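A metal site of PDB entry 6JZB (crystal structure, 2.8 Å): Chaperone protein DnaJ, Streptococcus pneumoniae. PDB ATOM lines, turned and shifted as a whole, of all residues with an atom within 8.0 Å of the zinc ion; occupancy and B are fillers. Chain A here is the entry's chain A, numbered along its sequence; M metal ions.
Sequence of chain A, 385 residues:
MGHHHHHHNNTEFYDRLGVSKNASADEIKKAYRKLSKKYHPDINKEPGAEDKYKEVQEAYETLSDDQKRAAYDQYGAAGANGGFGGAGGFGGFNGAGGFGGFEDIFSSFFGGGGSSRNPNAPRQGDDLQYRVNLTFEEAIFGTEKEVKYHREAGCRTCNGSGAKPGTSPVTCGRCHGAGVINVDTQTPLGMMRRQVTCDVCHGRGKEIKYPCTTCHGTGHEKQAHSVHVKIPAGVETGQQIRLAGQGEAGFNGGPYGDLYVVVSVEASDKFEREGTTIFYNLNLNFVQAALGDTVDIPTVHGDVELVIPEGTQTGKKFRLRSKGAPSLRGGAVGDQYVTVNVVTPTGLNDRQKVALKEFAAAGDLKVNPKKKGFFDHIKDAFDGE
Thr 157 touches the zinc ion (OG1 to ZN, 3.8 Å).
Five residues have an atom within 4 Å of the zinc ion: Cys 155, Thr 157, Cys 158, Cys 212 and Cys 215.
The backbone carbonyl oxygen of Cys 215 is in hydrogen-bond range of the side-chain hydroxyl of Thr 218 (3.5 Å).
The side-chain hydroxyl (OG1) of Thr 214 sits close to the side-chain sulfur (SG) of Cys 155 (3.0 Å).
The backbone carbonyl oxygen (O) of Gly 162 is in hydrogen-bond range of the backbone NH (N) of Cys 212 (2.9 Å).
The side-chain sulfur of Cys 215 lies close to the backbone NH of Gly 217 (3.6 Å).
The backbone NH (N) of Cys 155 lies within hydrogen-bond range of the backbone carbonyl oxygen (O) of Gly 219 (2.6 Å).
N of Gly 160 sits close to SG of Cys 158 (3.8 Å).
The side-chain sulfur (SG) of Cys 212 lies close to the side-chain hydroxyl (OG1) of Thr 157, at 3.2 Å.
N of Thr 214 sits close to SG of Cys 212.
The zinc ion is bound by SG of Cys 158 (2.1 Å).
The side-chain sulfur (SG) of Cys 215 binds the zinc ion, at 2.2 Å.
SG of Cys 212 is bound to the zinc ion.
The zinc ion is bound by the side-chain sulfur (SG) of Cys 155 (2.5 Å).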
ATOM      1  N   GLY A 154      34.903 -19.375  14.096  1.00  0.00           N
ATOM      2  CA  GLY A 154      34.418 -18.262  13.291  1.00  0.00           C
ATOM      3  C   GLY A 154      33.417 -18.621  12.220  1.00  0.00           C
ATOM      4  O   GLY A 154      33.795 -18.914  11.082  1.00  0.00           O
ATOM      5  N   CYS A 155      32.182 -18.158  12.410  1.00  0.00           N
ATOM      6  CA  CYS A 155      31.031 -18.809  11.787  1.00  0.00           C
ATOM      7  C   CYS A 155      31.163 -18.906  10.264  1.00  0.00           C
ATOM      8  O   CYS A 155      31.382 -17.901   9.592  1.00  0.00           O
ATOM      9  CB  CYS A 155      29.761 -18.039  12.141  1.00  0.00           C
ATOM     10  SG  CYS A 155      28.422 -19.046  12.788  1.00  0.00           S
ATOM     11  N   ARG A 156      31.039 -20.118   9.722  1.00  0.00           N
ATOM     12  CA  ARG A 156      30.848 -20.198   8.284  1.00  0.00           C
ATOM     13  C   ARG A 156      29.401 -19.867   7.939  1.00  0.00           C
ATOM     14  O   ARG A 156      29.126 -19.416   6.819  1.00  0.00           O
ATOM     15  CB  ARG A 156      31.271 -21.593   7.746  1.00  0.00           C
ATOM     16  CG  ARG A 156      31.360 -22.733   8.811  1.00  0.00           C
ATOM     17  CD  ARG A 156      31.845 -24.067   8.236  1.00  0.00           C
ATOM     18  NE  ARG A 156      31.830 -25.102   9.268  1.00  0.00           N
ATOM     19  CZ  ARG A 156      30.725 -25.704   9.709  1.00  0.00           C
ATOM     20  NH1 ARG A 156      29.539 -25.369   9.231  1.00  0.00           N
ATOM     21  NH2 ARG A 156      30.803 -26.622  10.650  1.00  0.00           N
ATOM     22  N   THR A 157      28.502 -20.024   8.917  1.00  0.00           N
ATOM     23  CA  THR A 157      27.079 -19.801   8.670  1.00  0.00           C
ATOM     24  C   THR A 157      26.803 -18.314   8.473  1.00  0.00           C
ATOM     25  O   THR A 157      25.848 -17.969   7.764  1.00  0.00           O
ATOM     26  CB  THR A 157      26.189 -20.363   9.819  1.00  0.00           C
ATOM     27  OG1 THR A 157      25.643 -19.274  10.589  1.00  0.00           O
ATOM     28  CG2 THR A 157      26.912 -21.316  10.760  1.00  0.00           C
ATOM     29  N   CYS A 158      27.513 -17.453   9.215  1.00  0.00           N
ATOM     30  CA  CYS A 158      27.425 -15.997   9.082  1.00  0.00           C
ATOM     31  C   CYS A 158      28.657 -15.271   8.488  1.00  0.00           C
ATOM     32  O   CYS A 158      28.663 -14.044   8.505  1.00  0.00           O
ATOM     33  CB  CYS A 158      27.068 -15.378  10.433  1.00  0.00           C
ATOM     34  SG  CYS A 158      28.314 -15.497  11.685  1.00  0.00           S
ATOM     35  N   ASN A 159      29.713 -15.964   8.035  1.00  0.00           N
ATOM     36  CA  ASN A 159      30.901 -15.317   7.526  1.00  0.00           C
ATOM     37  C   ASN A 159      31.645 -14.422   8.519  1.00  0.00           C
ATOM     38  O   ASN A 159      32.348 -13.492   8.135  1.00  0.00           O
ATOM     39  CB  ASN A 159      30.588 -14.568   6.256  1.00  0.00           C
ATOM     40  CG  ASN A 159      31.031 -15.315   5.029  1.00  0.00           C
ATOM     41  OD1 ASN A 159      31.716 -16.318   5.138  1.00  0.00           O
ATOM     42  ND2 ASN A 159      30.651 -14.831   3.870  1.00  0.00           N
ATOM     43  N   GLY A 160      31.509 -14.730   9.794  1.00  0.00           N
ATOM     44  CA  GLY A 160      32.200 -14.006  10.848  1.00  0.00           C
ATOM     45  C   GLY A 160      31.542 -12.823  11.523  1.00  0.00           C
ATOM     46  O   GLY A 160      31.992 -12.393  12.566  1.00  0.00           O
ATOM     47  N   SER A 161      30.464 -12.328  10.955  1.00  0.00           N
ATOM     48  CA  SER A 161      29.725 -11.208  11.540  1.00  0.00           C
ATOM     49  C   SER A 161      28.488 -11.883  12.054  1.00  0.00           C
ATOM     50  O   SER A 161      27.809 -12.556  11.281  1.00  0.00           O
ATOM     51  CB  SER A 161      29.345 -10.228  10.478  1.00  0.00           C
ATOM     52  OG  SER A 161      28.770 -10.922   9.395  1.00  0.00           O
ATOM     53  N   GLY A 162      28.124 -11.670  13.304  1.00  0.00           N
ATOM     54  CA  GLY A 162      27.018 -12.425  13.847  1.00  0.00           C
ATOM     55  C   GLY A 162      25.654 -11.938  13.449  1.00  0.00           C
ATOM     56  O   GLY A 162      24.821 -11.688  14.294  1.00  0.00           O
ATOM     57  N   ALA A 163      25.394 -11.919  12.151  1.00  0.00           N
ATOM     58  CA  ALA A 163      24.099 -11.470  11.675  1.00  0.00           C
ATOM     59  C   ALA A 163      23.426 -12.466  10.766  1.00  0.00           C
ATOM     60  O   ALA A 163      24.045 -12.964   9.846  1.00  0.00           O
ATOM     61  CB  ALA A 163      24.262 -10.160  10.952  1.00  0.00           C
ATOM     62  N   LYS A 164      22.158 -12.728  11.006  1.00  0.00           N
ATOM     63  CA  LYS A 164      21.435 -13.682  10.165  1.00  0.00           C
ATOM     64  C   LYS A 164      21.726 -13.388   8.722  1.00  0.00           C
ATOM     65  O   LYS A 164      21.517 -12.273   8.271  1.00  0.00           O
ATOM     66  CB  LYS A 164      19.939 -13.607  10.428  1.00  0.00           C
ATOM     67  CG  LYS A 164      19.105 -14.579   9.610  1.00  0.00           C
ATOM     68  CD  LYS A 164      17.687 -14.707  10.152  1.00  0.00           C
ATOM     69  CE  LYS A 164      16.634 -14.537   9.068  1.00  0.00           C
ATOM     70  NZ  LYS A 164      15.323 -13.998   9.550  1.00  0.00           N
ATOM     71  N   PRO A 165      22.215 -14.375   7.985  1.00  0.00           N
ATOM     72  CA  PRO A 165      22.578 -14.050   6.604  1.00  0.00           C
ATOM     73  C   PRO A 165      21.422 -13.333   5.936  1.00  0.00           C
ATOM     74  O   PRO A 165      20.259 -13.569   6.255  1.00  0.00           O
ATOM     75  CB  PRO A 165      22.833 -15.421   5.970  1.00  0.00           C
ATOM     76  CG  PRO A 165      23.134 -16.324   7.123  1.00  0.00           C
ATOM     77  CD  PRO A 165      22.369 -15.802   8.296  1.00  0.00           C
ATOM     78  N   PRO A 211      20.650 -11.377  14.712  1.00  0.00           N
ATOM     79  CA  PRO A 211      21.944 -12.066  14.779  1.00  0.00           C
ATOM     80  C   PRO A 211      21.893 -13.478  14.203  1.00  0.00           C
ATOM     81  O   PRO A 211      20.830 -14.099  14.106  1.00  0.00           O
ATOM     82  CB  PRO A 211      22.204 -12.127  16.282  1.00  0.00           C
ATOM     83  CG  PRO A 211      20.859 -12.334  16.850  1.00  0.00           C
ATOM     84  CD  PRO A 211      19.883 -11.576  15.951  1.00  0.00           C
ATOM     85  N   CYS A 212      23.069 -13.980  13.843  1.00  0.00           N
ATOM     86  CA  CYS A 212      23.186 -15.335  13.323  1.00  0.00           C
ATOM     87  C   CYS A 212      22.739 -16.360  14.361  1.00  0.00           C
ATOM     88  O   CYS A 212      22.970 -16.211  15.570  1.00  0.00           O
ATOM     89  CB  CYS A 212      24.608 -15.633  12.890  1.00  0.00           C
ATOM     90  SG  CYS A 212      25.060 -17.364  13.038  1.00  0.00           S
ATOM     91  N   THR A 213      22.117 -17.432  13.871  1.00  0.00           N
ATOM     92  CA  THR A 213      21.399 -18.369  14.725  1.00  0.00           C
ATOM     93  C   THR A 213      22.343 -19.274  15.515  1.00  0.00           C
ATOM     94  O   THR A 213      22.052 -19.616  16.680  1.00  0.00           O
ATOM     95  CB  THR A 213      20.492 -19.231  13.846  1.00  0.00           C
ATOM     96  OG1 THR A 213      21.256 -20.327  13.314  1.00  0.00           O
ATOM     97  CG2 THR A 213      19.923 -18.403  12.679  1.00  0.00           C
ATOM     98  N   THR A 214      23.458 -19.652  14.907  1.00  0.00           N
ATOM     99  CA  THR A 214      24.328 -20.699  15.443  1.00  0.00           C
ATOM    100  C   THR A 214      25.334 -20.125  16.439  1.00  0.00           C
ATOM    101  O   THR A 214      25.546 -20.698  17.510  1.00  0.00           O
ATOM    102  CB  THR A 214      25.048 -21.391  14.283  1.00  0.00           C
ATOM    103  OG1 THR A 214      26.278 -20.709  13.998  1.00  0.00           O
ATOM    104  CG2 THR A 214      24.168 -21.373  13.021  1.00  0.00           C
ATOM    105  N   CYS A 215      25.920 -18.982  16.098  1.00  0.00           N
ATOM    106  CA  CYS A 215      26.931 -18.315  16.915  1.00  0.00           C
ATOM    107  C   CYS A 215      26.348 -17.294  17.878  1.00  0.00           C
ATOM    108  O   CYS A 215      27.108 -16.525  18.467  1.00  0.00           O
ATOM    109  CB  CYS A 215      27.950 -17.642  16.006  1.00  0.00           C
ATOM    110  SG  CYS A 215      27.216 -16.316  15.121  1.00  0.00           S
ATOM    111  N   HIS A 216      25.021 -17.210  17.987  1.00  0.00           N
ATOM    112  CA  HIS A 216      24.339 -16.277  18.883  1.00  0.00           C
ATOM    113  C   HIS A 216      24.900 -14.855  18.804  1.00  0.00           C
ATOM    114  O   HIS A 216      24.866 -14.130  19.802  1.00  0.00           O
ATOM    115  CB  HIS A 216      24.411 -16.764  20.324  1.00  0.00           C
ATOM    116  CG  HIS A 216      24.269 -18.248  20.486  1.00  0.00           C
ATOM    117  ND1 HIS A 216      25.309 -19.129  20.269  1.00  0.00           N
ATOM    118  CD2 HIS A 216      23.209 -18.994  20.859  1.00  0.00           C
ATOM    119  CE1 HIS A 216      24.891 -20.365  20.509  1.00  0.00           C
ATOM    120  NE2 HIS A 216      23.618 -20.315  20.863  1.00  0.00           N
ATOM    121  N   GLY A 217      25.458 -14.449  17.667  1.00  0.00           N
ATOM    122  CA  GLY A 217      25.863 -13.073  17.491  1.00  0.00           C
ATOM    123  C   GLY A 217      27.341 -12.778  17.423  1.00  0.00           C
ATOM    124  O   GLY A 217      27.784 -12.018  16.554  1.00  0.00           O
ATOM    125  N   THR A 218      28.147 -13.332  18.347  1.00  0.00           N
ATOM    126  CA  THR A 218      29.597 -13.253  18.243  1.00  0.00           C
ATOM    127  C   THR A 218      30.055 -14.192  17.157  1.00  0.00           C
ATOM    128  O   THR A 218      29.631 -15.356  17.124  1.00  0.00           O
ATOM    129  CB  THR A 218      30.276 -13.639  19.546  1.00  0.00           C
ATOM    130  OG1 THR A 218      29.737 -14.897  20.006  1.00  0.00           O
ATOM    131  CG2 THR A 218      30.142 -12.525  20.632  1.00  0.00           C
ATOM    132  N   GLY A 219      30.916 -13.708  16.276  1.00  0.00           N
ATOM    133  CA  GLY A 219      31.181 -14.423  15.046  1.00  0.00           C
ATOM    134  C   GLY A 219      31.876 -15.789  15.144  1.00  0.00           C
ATOM    135  O   GLY A 219      32.461 -16.201  14.145  1.00  0.00           O
ATOM    136  N   HIS A 220      31.801 -16.511  16.273  1.00  0.00           N
ATOM    137  CA  HIS A 220      32.682 -17.654  16.517  1.00  0.00           C
ATOM    138  C   HIS A 220      31.865 -18.917  16.749  1.00  0.00           C
ATOM    139  O   HIS A 220      31.166 -19.051  17.768  1.00  0.00           O
ATOM    140  CB  HIS A 220      33.628 -17.387  17.691  1.00  0.00           C
ATOM    141  CG  HIS A 220      34.786 -16.493  17.336  1.00  0.00           C
ATOM    142  ND1 HIS A 220      35.745 -16.109  18.246  1.00  0.00           N
ATOM    143  CD2 HIS A 220      35.120 -15.890  16.163  1.00  0.00           C
ATOM    144  CE1 HIS A 220      36.622 -15.320  17.648  1.00  0.00           C
ATOM    145  NE2 HIS A 220      36.264 -15.176  16.380  1.00  0.00           N
ATOM    146  N   GLU A 221      31.989 -19.851  15.811  1.00  0.00           N
ATOM    147  CA  GLU A 221      31.338 -21.145  15.847  1.00  0.00           C
ATOM    148  C   GLU A 221      32.305 -22.176  16.422  1.00  0.00           C
ATOM    149  O   GLU A 221      33.512 -22.096  16.160  1.00  0.00           O
ATOM    150  CB  GLU A 221      30.905 -21.569  14.446  1.00  0.00           C
ATOM    151  CG  GLU A 221      30.166 -22.887  14.372  1.00  0.00           C
ATOM    152  CD  GLU A 221      29.971 -23.383  12.945  1.00  0.00           C
ATOM    153  OE1 GLU A 221      30.188 -22.609  11.977  1.00  0.00           O
ATOM    154  OE2 GLU A 221      29.613 -24.576  12.791  1.00  0.00           O
HETATM  155 ZN    ZN M   1      27.277 -16.825  12.957  1.00  0.00          ZN
